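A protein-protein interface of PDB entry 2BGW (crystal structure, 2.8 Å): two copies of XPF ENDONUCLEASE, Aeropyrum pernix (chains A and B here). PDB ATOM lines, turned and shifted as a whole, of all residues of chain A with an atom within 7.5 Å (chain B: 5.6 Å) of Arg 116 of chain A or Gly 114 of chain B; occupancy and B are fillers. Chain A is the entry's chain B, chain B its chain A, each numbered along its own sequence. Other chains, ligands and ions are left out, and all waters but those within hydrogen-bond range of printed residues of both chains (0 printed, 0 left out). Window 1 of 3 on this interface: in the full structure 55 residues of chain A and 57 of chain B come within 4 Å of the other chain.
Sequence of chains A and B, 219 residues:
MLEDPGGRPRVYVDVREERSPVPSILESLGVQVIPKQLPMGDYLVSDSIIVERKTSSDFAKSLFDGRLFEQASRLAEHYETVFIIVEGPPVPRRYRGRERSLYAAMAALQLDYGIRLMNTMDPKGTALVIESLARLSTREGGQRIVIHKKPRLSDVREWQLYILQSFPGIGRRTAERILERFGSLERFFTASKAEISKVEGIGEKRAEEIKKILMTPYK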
ATOM      1  N   ILE A  50      26.713 -32.268 -34.240  1.00  0.00           N
ATOM      2  CA  ILE A  50      25.402 -32.567 -34.772  1.00  0.00           C
ATOM      3  C   ILE A  50      24.290 -31.868 -34.005  1.00  0.00           C
ATOM      4  O   ILE A  50      24.344 -31.720 -32.778  1.00  0.00           O
ATOM      5  CB  ILE A  50      25.137 -34.062 -34.780  1.00  0.00           C
ATOM      6  CG1 ILE A  50      23.840 -34.366 -35.545  1.00  0.00           C
ATOM      7  CG2 ILE A  50      25.073 -34.590 -33.347  1.00  0.00           C
ATOM      8  CD1 ILE A  50      24.011 -35.289 -36.713  1.00  0.00           C
ATOM      9  N   GLU A  52      20.091 -31.701 -33.273  1.00  0.00           N
ATOM     10  CA  GLU A  52      18.836 -32.411 -33.243  1.00  0.00           C
ATOM     11  C   GLU A  52      17.748 -31.386 -32.964  1.00  0.00           C
ATOM     12  O   GLU A  52      17.825 -30.634 -31.979  1.00  0.00           O
ATOM     13  CB  GLU A  52      18.885 -33.466 -32.140  1.00  0.00           C
ATOM     14  CG  GLU A  52      17.592 -34.164 -31.812  1.00  0.00           C
ATOM     15  CD  GLU A  52      16.946 -34.864 -33.005  1.00  0.00           C
ATOM     16  OE1 GLU A  52      17.660 -35.319 -33.951  1.00  0.00           O
ATOM     17  OE2 GLU A  52      15.696 -34.970 -32.972  1.00  0.00           O
ATOM     18  N   GLU A  80      30.987 -36.198 -31.224  1.00  0.00           N
ATOM     19  CA  GLU A  80      31.642 -35.561 -30.056  1.00  0.00           C
ATOM     20  C   GLU A  80      30.726 -34.535 -29.363  1.00  0.00           C
ATOM     21  O   GLU A  80      30.620 -34.528 -28.165  1.00  0.00           O
ATOM     22  CB  GLU A  80      33.001 -34.928 -30.427  1.00  0.00           C
ATOM     23  CG  GLU A  80      33.851 -34.474 -29.235  1.00  0.00           C
ATOM     24  N   THR A  81      30.058 -33.679 -30.120  1.00  0.00           N
ATOM     25  CA  THR A  81      29.233 -32.639 -29.532  1.00  0.00           C
ATOM     26  C   THR A  81      27.820 -32.806 -30.064  1.00  0.00           C
ATOM     27  O   THR A  81      27.629 -33.000 -31.253  1.00  0.00           O
ATOM     28  CB  THR A  81      29.816 -31.230 -29.857  1.00  0.00           C
ATOM     29  OG1 THR A  81      31.055 -31.090 -29.183  1.00  0.00           O
ATOM     30  CG2 THR A  81      28.935 -30.118 -29.345  1.00  0.00           C
ATOM     31  N   VAL A  82      26.832 -32.733 -29.180  1.00  0.00           N
ATOM     32  CA  VAL A  82      25.451 -32.951 -29.574  1.00  0.00           C
ATOM     33  C   VAL A  82      24.596 -31.838 -29.052  1.00  0.00           C
ATOM     34  O   VAL A  82      24.599 -31.563 -27.848  1.00  0.00           O
ATOM     35  CB  VAL A  82      24.896 -34.284 -29.026  1.00  0.00           C
ATOM     36  CG1 VAL A  82      23.410 -34.394 -29.306  1.00  0.00           C
ATOM     37  CG2 VAL A  82      25.660 -35.488 -29.622  1.00  0.00           C
ATOM     38  N   PHE A  83      23.853 -31.196 -29.957  1.00  0.00           N
ATOM     39  CA  PHE A  83      22.834 -30.207 -29.560  1.00  0.00           C
ATOM     40  C   PHE A  83      21.440 -30.724 -29.814  1.00  0.00           C
ATOM     41  O   PHE A  83      21.172 -31.315 -30.865  1.00  0.00           O
ATOM     42  CB  PHE A  83      23.006 -28.928 -30.350  1.00  0.00           C
ATOM     43  CG  PHE A  83      24.174 -28.125 -29.933  1.00  0.00           C
ATOM     44  CD1 PHE A  83      25.416 -28.358 -30.491  1.00  0.00           C
ATOM     45  CD2 PHE A  83      24.028 -27.119 -28.994  1.00  0.00           C
ATOM     46  CE1 PHE A  83      26.489 -27.619 -30.126  1.00  0.00           C
ATOM     47  CE2 PHE A  83      25.107 -26.368 -28.620  1.00  0.00           C
ATOM     48  CZ  PHE A  83      26.347 -26.636 -29.182  1.00  0.00           C
ATOM     49  N   ILE A  84      20.543 -30.498 -28.870  1.00  0.00           N
ATOM     50  CA  ILE A  84      19.136 -30.711 -29.137  1.00  0.00           C
ATOM     51  C   ILE A  84      18.544 -29.343 -29.000  1.00  0.00           C
ATOM     52  O   ILE A  84      18.632 -28.749 -27.940  1.00  0.00           O
ATOM     53  CB  ILE A  84      18.502 -31.713 -28.165  1.00  0.00           C
ATOM     54  CG1 ILE A  84      19.015 -33.119 -28.492  1.00  0.00           C
ATOM     55  CG2 ILE A  84      17.002 -31.692 -28.275  1.00  0.00           C
ATOM     56  CD1 ILE A  84      18.723 -34.181 -27.456  1.00  0.00           C
ATOM     57  N   ILE A  85      18.003 -28.813 -30.096  1.00  0.00           N
ATOM     58  CA  ILE A  85      17.333 -27.514 -30.068  1.00  0.00           C
ATOM     59  C   ILE A  85      15.852 -27.796 -29.904  1.00  0.00           C
ATOM     60  O   ILE A  85      15.245 -28.459 -30.751  1.00  0.00           O
ATOM     61  CB  ILE A  85      17.585 -26.686 -31.358  1.00  0.00           C
ATOM     62  CG1 ILE A  85      19.070 -26.615 -31.677  1.00  0.00           C
ATOM     63  CG2 ILE A  85      17.038 -25.262 -31.209  1.00  0.00           C
ATOM     64  CD1 ILE A  85      19.360 -26.078 -33.059  1.00  0.00           C
ATOM     65  N   VAL A  86      15.289 -27.320 -28.806  1.00  0.00           N
ATOM     66  CA  VAL A  86      13.907 -27.592 -28.480  1.00  0.00           C
ATOM     67  C   VAL A  86      13.118 -26.339 -28.782  1.00  0.00           C
ATOM     68  O   VAL A  86      13.277 -25.306 -28.128  1.00  0.00           O
ATOM     69  CB  VAL A  86      13.763 -28.042 -27.007  1.00  0.00           C
ATOM     70  CG1 VAL A  86      12.325 -27.978 -26.524  1.00  0.00           C
ATOM     71  CG2 VAL A  86      14.310 -29.444 -26.848  1.00  0.00           C
ATOM     72  N   LEU A 109      19.918 -35.255 -19.538  1.00  0.00           N
ATOM     73  CA  LEU A 109      20.500 -35.224 -20.867  1.00  0.00           C
ATOM     74  C   LEU A 109      21.867 -34.559 -20.805  1.00  0.00           C
ATOM     75  O   LEU A 109      22.818 -35.047 -21.397  1.00  0.00           O
ATOM     76  CB  LEU A 109      19.576 -34.578 -21.898  1.00  0.00           C
ATOM     77  CG  LEU A 109      18.395 -35.432 -22.356  1.00  0.00           C
ATOM     78  CD1 LEU A 109      17.320 -34.536 -22.910  1.00  0.00           C
ATOM     79  CD2 LEU A 109      18.823 -36.438 -23.383  1.00  0.00           C
ATOM     80  N   GLN A 110      21.975 -33.483 -20.044  1.00  0.00           N
ATOM     81  CA  GLN A 110      23.255 -32.796 -19.921  1.00  0.00           C
ATOM     82  C   GLN A 110      24.350 -33.474 -19.053  1.00  0.00           C
ATOM     83  O   GLN A 110      25.486 -33.603 -19.498  1.00  0.00           O
ATOM     84  CB  GLN A 110      23.038 -31.371 -19.482  1.00  0.00           C
ATOM     85  CG  GLN A 110      22.070 -30.669 -20.358  1.00  0.00           C
ATOM     86  CD  GLN A 110      22.453 -29.252 -20.580  1.00  0.00           C
ATOM     87  OE1 GLN A 110      23.560 -28.962 -21.021  1.00  0.00           O
ATOM     88  NE2 GLN A 110      21.528 -28.341 -20.288  1.00  0.00           N
ATOM     89  N   TYR A 113      24.727 -37.531 -20.520  1.00  0.00           N
ATOM     90  CA  TYR A 113      24.917 -37.789 -21.943  1.00  0.00           C
ATOM     91  C   TYR A 113      25.768 -36.709 -22.520  1.00  0.00           C
ATOM     92  O   TYR A 113      26.289 -36.844 -23.628  1.00  0.00           O
ATOM     93  CB  TYR A 113      23.590 -37.833 -22.686  1.00  0.00           C
ATOM     94  CG  TYR A 113      22.821 -39.113 -22.485  1.00  0.00           C
ATOM     95  CD1 TYR A 113      21.742 -39.158 -21.612  1.00  0.00           C
ATOM     96  CD2 TYR A 113      23.181 -40.285 -23.167  1.00  0.00           C
ATOM     97  CE1 TYR A 113      21.034 -40.337 -21.425  1.00  0.00           C
ATOM     98  CE2 TYR A 113      22.486 -41.470 -22.983  1.00  0.00           C
ATOM     99  CZ  TYR A 113      21.411 -41.485 -22.109  1.00  0.00           C
ATOM    100  OH  TYR A 113      20.709 -42.646 -21.914  1.00  0.00           O
ATOM    101  N   GLY A 114      25.906 -35.629 -21.763  1.00  0.00           N
ATOM    102  CA  GLY A 114      26.785 -34.561 -22.156  1.00  0.00           C
ATOM    103  C   GLY A 114      26.146 -33.696 -23.191  1.00  0.00           C
ATOM    104  O   GLY A 114      26.718 -32.712 -23.594  1.00  0.00           O
ATOM    105  N   ILE A 115      24.951 -34.069 -23.613  1.00  0.00           N
ATOM    106  CA  ILE A 115      24.197 -33.357 -24.611  1.00  0.00           C
ATOM    107  C   ILE A 115      23.889 -31.915 -24.201  1.00  0.00           C
ATOM    108  O   ILE A 115      23.611 -31.624 -23.038  1.00  0.00           O
ATOM    109  CB  ILE A 115      22.926 -34.158 -24.868  1.00  0.00           C
ATOM    110  CG1 ILE A 115      23.253 -35.297 -25.813  1.00  0.00           C
ATOM    111  CG2 ILE A 115      21.791 -33.319 -25.431  1.00  0.00           C
ATOM    112  CD1 ILE A 115      22.226 -36.377 -25.760  1.00  0.00           C
ATOM    113  N   ARG A 116      23.926 -31.012 -25.169  1.00  0.00           N
ATOM    114  CA  ARG A 116      23.640 -29.609 -24.907  1.00  0.00           C
ATOM    115  C   ARG A 116      22.296 -29.201 -25.444  1.00  0.00           C
ATOM    116  O   ARG A 116      21.921 -29.564 -26.548  1.00  0.00           O
ATOM    117  CB  ARG A 116      24.731 -28.731 -25.505  1.00  0.00           C
ATOM    118  CG  ARG A 116      26.095 -29.089 -24.980  1.00  0.00           C
ATOM    119  CD  ARG A 116      27.152 -28.254 -25.599  1.00  0.00           C
ATOM    120  NE  ARG A 116      27.858 -27.531 -24.547  1.00  0.00           N
ATOM    121  CZ  ARG A 116      28.916 -28.014 -23.940  1.00  0.00           C
ATOM    122  NH1 ARG A 116      29.385 -29.197 -24.305  1.00  0.00           N
ATOM    123  NH2 ARG A 116      29.487 -27.325 -22.984  1.00  0.00           N
ATOM    124  N   LEU A 117      21.571 -28.435 -24.663  1.00  0.00           N
ATOM    125  CA  LEU A 117      20.259 -28.026 -25.068  1.00  0.00           C
ATOM    126  C   LEU A 117      20.213 -26.563 -25.441  1.00  0.00           C
ATOM    127  O   LEU A 117      20.875 -25.728 -24.834  1.00  0.00           O
ATOM    128  CB  LEU A 117      19.312 -28.219 -23.913  1.00  0.00           C
ATOM    129  CG  LEU A 117      19.276 -29.628 -23.377  1.00  0.00           C
ATOM    130  CD1 LEU A 117      18.257 -29.610 -22.294  1.00  0.00           C
ATOM    131  CD2 LEU A 117      18.888 -30.616 -24.459  1.00  0.00           C
ATOM    132  N   MET A 118      19.396 -26.222 -26.419  1.00  0.00           N
ATOM    133  CA  MET A 118      19.047 -24.833 -26.573  1.00  0.00           C
ATOM    134  C   MET A 118      17.547 -24.818 -26.511  1.00  0.00           C
ATOM    135  O   MET A 118      16.892 -25.823 -26.774  1.00  0.00           O
ATOM    136  CB  MET A 118      19.543 -24.290 -27.902  1.00  0.00           C
ATOM    137  CG  MET A 118      20.989 -24.647 -28.218  1.00  0.00           C
ATOM    138  SD  MET A 118      22.158 -23.326 -27.940  1.00  0.00           S
ATOM    139  CE  MET A 118      21.235 -22.283 -26.818  1.00  0.00           C
ATOM    140  N   VAL B  82      29.636 -25.539 -16.020  1.00  0.00           N
ATOM    141  CA  VAL B  82      28.910 -24.300 -15.755  1.00  0.00           C
ATOM    142  C   VAL B  82      27.529 -24.369 -16.374  1.00  0.00           C
ATOM    143  O   VAL B  82      27.399 -24.555 -17.567  1.00  0.00           O
ATOM    144  CB  VAL B  82      29.659 -23.056 -16.354  1.00  0.00           C
ATOM    145  CG1 VAL B  82      28.969 -21.794 -15.958  1.00  0.00           C
ATOM    146  CG2 VAL B  82      31.084 -22.999 -15.879  1.00  0.00           C
ATOM    147  N   ALA B 108      27.546 -19.045 -28.609  1.00  0.00           N
ATOM    148  CA  ALA B 108      28.942 -18.716 -28.233  1.00  0.00           C
ATOM    149  C   ALA B 108      29.319 -19.116 -26.801  1.00  0.00           C
ATOM    150  O   ALA B 108      30.397 -19.687 -26.585  1.00  0.00           O
ATOM    151  CB  ALA B 108      29.236 -17.220 -28.454  1.00  0.00           C
ATOM    152  N   LEU B 109      28.454 -18.798 -25.829  1.00  0.00           N
ATOM    153  CA  LEU B 109      28.642 -19.241 -24.456  1.00  0.00           C
ATOM    154  C   LEU B 109      28.842 -20.743 -24.432  1.00  0.00           C
ATOM    155  O   LEU B 109      29.599 -21.255 -23.623  1.00  0.00           O
ATOM    156  CB  LEU B 109      27.429 -18.938 -23.635  1.00  0.00           C
ATOM    157  CG  LEU B 109      27.134 -17.485 -23.381  1.00  0.00           C
ATOM    158  CD1 LEU B 109      25.708 -17.396 -22.967  1.00  0.00           C
ATOM    159  CD2 LEU B 109      28.016 -16.967 -22.295  1.00  0.00           C
ATOM    160  N   GLN B 110      28.165 -21.437 -25.346  1.00  0.00           N
ATOM    161  CA  GLN B 110      28.186 -22.882 -25.431  1.00  0.00           C
ATOM    162  C   GLN B 110      29.422 -23.394 -26.136  1.00  0.00           C
ATOM    163  O   GLN B 110      30.008 -24.349 -25.695  1.00  0.00           O
ATOM    164  CB  GLN B 110      26.953 -23.383 -26.178  1.00  0.00           C
ATOM    165  CG  GLN B 110      25.650 -23.527 -25.360  1.00  0.00           C
ATOM    166  CD  GLN B 110      25.504 -24.925 -24.806  1.00  0.00           C
ATOM    167  OE1 GLN B 110      26.490 -25.526 -24.339  1.00  0.00           O
ATOM    168  NE2 GLN B 110      24.287 -25.461 -24.849  1.00  0.00           N
ATOM    169  N   LEU B 111      29.818 -22.791 -27.244  1.00  0.00           N
ATOM    170  CA  LEU B 111      30.968 -23.301 -27.998  1.00  0.00           C
ATOM    171  C   LEU B 111      32.312 -22.713 -27.561  1.00  0.00           C
ATOM    172  O   LEU B 111      33.336 -23.375 -27.624  1.00  0.00           O
ATOM    173  CB  LEU B 111      30.791 -23.059 -29.497  1.00  0.00           C
ATOM    174  CG  LEU B 111      29.941 -23.981 -30.369  1.00  0.00           C
ATOM    175  CD1 LEU B 111      30.364 -23.863 -31.844  1.00  0.00           C
ATOM    176  CD2 LEU B 111      30.060 -25.419 -29.909  1.00  0.00           C
ATOM    177  N   ASP B 112      32.308 -21.458 -27.142  1.00  0.00           N
ATOM    178  CA  ASP B 112      33.545 -20.766 -26.798  1.00  0.00           C
ATOM    179  C   ASP B 112      34.126 -21.175 -25.439  1.00  0.00           C
ATOM    180  O   ASP B 112      35.318 -21.382 -25.320  1.00  0.00           O
ATOM    181  CB  ASP B 112      33.329 -19.240 -26.838  1.00  0.00           C
ATOM    182  CG  ASP B 112      33.366 -18.670 -28.263  1.00  0.00           C
ATOM    183  OD1 ASP B 112      33.680 -19.427 -29.252  1.00  0.00           O
ATOM    184  OD2 ASP B 112      33.074 -17.444 -28.369  1.00  0.00           O
ATOM    185  N   TYR B 113      33.286 -21.273 -24.417  1.00  0.00           N
ATOM    186  CA  TYR B 113      33.764 -21.687 -23.126  1.00  0.00           C
ATOM    187  C   TYR B 113      33.063 -22.932 -22.559  1.00  0.00           C
ATOM    188  O   TYR B 113      33.086 -23.151 -21.343  1.00  0.00           O
ATOM    189  CB  TYR B 113      33.640 -20.556 -22.113  1.00  0.00           C
ATOM    190  CG  TYR B 113      33.831 -19.129 -22.590  1.00  0.00           C
ATOM    191  CD1 TYR B 113      32.722 -18.334 -22.864  1.00  0.00           C
ATOM    192  CD2 TYR B 113      35.091 -18.540 -22.673  1.00  0.00           C
ATOM    193  CE1 TYR B 113      32.842 -16.999 -23.251  1.00  0.00           C
ATOM    194  CE2 TYR B 113      35.231 -17.178 -23.071  1.00  0.00           C
ATOM    195  CZ  TYR B 113      34.079 -16.417 -23.360  1.00  0.00           C
ATOM    196  OH  TYR B 113      34.120 -15.084 -23.773  1.00  0.00           O
ATOM    197  N   GLY B 114      32.452 -23.743 -23.417  1.00  0.00           N
ATOM    198  CA  GLY B 114      31.714 -24.920 -22.981  1.00  0.00           C
ATOM    199  C   GLY B 114      30.599 -24.746 -21.950  1.00  0.00           C
ATOM    200  O   GLY B 114      30.188 -25.729 -21.336  1.00  0.00           O
ATOM    201  N   ILE B 115      30.098 -23.526 -21.736  1.00  0.00           N
ATOM    202  CA  ILE B 115      29.039 -23.323 -20.753  1.00  0.00           C
ATOM    203  C   ILE B 115      27.828 -24.073 -21.232  1.00  0.00           C
ATOM    204  O   ILE B 115      27.717 -24.364 -22.422  1.00  0.00           O
ATOM    205  CB  ILE B 115      28.728 -21.846 -20.533  1.00  0.00           C
ATOM    206  CG1 ILE B 115      29.729 -21.239 -19.568  1.00  0.00           C
ATOM    207  CG2 ILE B 115      27.368 -21.636 -19.901  1.00  0.00           C
ATOM    208  CD1 ILE B 115      30.708 -20.309 -20.240  1.00  0.00           C
ATOM    209  N   ARG B 116      26.953 -24.430 -20.294  1.00  0.00           N
ATOM    210  CA  ARG B 116      25.733 -25.214 -20.573  1.00  0.00           C
ATOM    211  C   ARG B 116      24.496 -24.410 -20.220  1.00  0.00           C
ATOM    212  O   ARG B 116      24.440 -23.769 -19.156  1.00  0.00           O
ATOM    213  CB  ARG B 116      25.759 -26.551 -19.823  1.00  0.00           C
ATOM    214  CG  ARG B 116      26.787 -27.481 -20.385  1.00  0.00           C
ATOM    215  CD  ARG B 116      26.995 -28.702 -19.562  1.00  0.00           C
ATOM    216  NE  ARG B 116      27.868 -29.644 -20.256  1.00  0.00           N
ATOM    217  CZ  ARG B 116      27.432 -30.514 -21.161  1.00  0.00           C
ATOM    218  NH1 ARG B 116      26.147 -30.545 -21.473  1.00  0.00           N
ATOM    219  NH2 ARG B 116      28.268 -31.342 -21.773  1.00  0.00           N
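The backbone NH of Glu 52 of chain A is in hydrogen-bond range of the backbone carbonyl oxygen of Phe 83 of chain A (2.7 Å). The backbone NH (N) of Arg 116 of chain B sits at hydrogen-bond distance from the backbone carbonyl oxygen (O) of Val 82 of chain B (2.8 Å). The backbone carbonyl oxygen of Leu 109 of chain A sits at hydrogen-bond distance from the backbone NH of Gly 114 of chain A (3.2 Å). O of Leu 109 of chain B is in hydrogen-bond range of N of Ile 115 of chain B. The backbone carbonyl oxygen (O) of Val 82 of chain A sits at hydrogen-bond distance from the backbone NH (N) of Arg 116 of chain A. OE1 of Gln 110 of chain B lies close to O of Ile 115 of chain B.
Of the 17 printed residues of chain A, 6 touch a printed residue of chain B. Printed residues of chain A that touch a printed residue of chain B: Phe 83, Gln 110, Gly 114, Ile 115, Arg 116 and Leu 117. Hydrophobic or aromatic side chains of chain A within 4 Å of the printed part of chain B: Phe 83. Printed residues of chain B that touch a printed residue of chain A: Gln 110, Leu 111, Gly 114, Ile 115 and Arg 116. Among the printed residues, no Asp or Glu carboxylate lies within 4 Å of a Lys or Arg side-chain nitrogen of the other chain.
The side-chain amide oxygen of Gln 110 of chain A lies within hydrogen-bond range of the guanidinium group of Arg 116 of chain B (3.1 Å). The guanidinium group of Arg 116 of chain B lies within hydrogen-bond range of the backbone carbonyl oxygen of Ile 115 of chain A (3.2 Å). The guanidinium group of Arg 116 of chain B is in hydrogen-bond range of the backbone carbonyl oxygen of Gly 114 of chain A, 2.8 Å away. The backbone carbonyl oxygen (O) of Ile 115 of chain B lies within hydrogen-bond range of the guanidinium group (NH2) of Arg 116 of chain A. The side-chain amide nitrogen (NE2) of Gln 110 of chain B sits at hydrogen-bond distance from the backbone carbonyl oxygen (O) of Leu 117 of chain A (3.4 Å). The backbone carbonyl oxygen of Gly 114 of chain B sits close to the guanidinium group of Arg 116 of chain A (2.4 Å). NE of Arg 116 of chain A is in hydrogen-bond range of OE1 of Gln 110 of chain B (2.4 Å).
Gln 110 of chain A touches Arg 116 of chain B, and with the chains exchanged Arg 116 of chain A touches Gln 110 of chain B. Gly 114 of chain A touches Arg 116 of chain B, and with the chains exchanged Arg 116 of chain A touches Gly 114 of chain B. Ile 115 of chain A touches Arg 116 of chain B, and with the chains exchanged Arg 116 of chain A touches Ile 115 of chain B. Arg 116 of chain A touches its own counterpart, Arg 116 of chain B. Positions printed for both chains: 82, 109, 110, 113, 114, 115 and 116.
Among the printed residues, pairs that only touch across the chains: Arg 116 of chain A with Arg 116 of chain B, Phe 83 of chain A with Gln 110 of chain B and Phe 83 of chain A with Leu 111 of chain B.
Arg 116 of chain A touches four residues of chain B. Gly 114 of chain B touches one residue of chain A. Printed residues of chain B within 4 Å of Leu 117 of chain A: Gln 110 (3.4 Å). Of the printed residues of chain A, Gln 110 of chain B touches Phe 83 (3.96 Å), Arg 116 (2.4 Å) and Leu 117 (3.4 Å). Of the printed residues of chain B, Phe 83 of chain A touches Gln 110 and Leu 111. Of the printed residues of chain A, Arg 116 of chain B touches Gln 110 (3.1 Å), Gly 114 (2.8 Å), Ile 115 (3.2 Å) and Arg 116 (3.5 Å). Printed residues of chain B within 4 Å of Gln 110 of chain A: Arg 116. Val 82 of chain A touches none of the printed residues of chain B.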
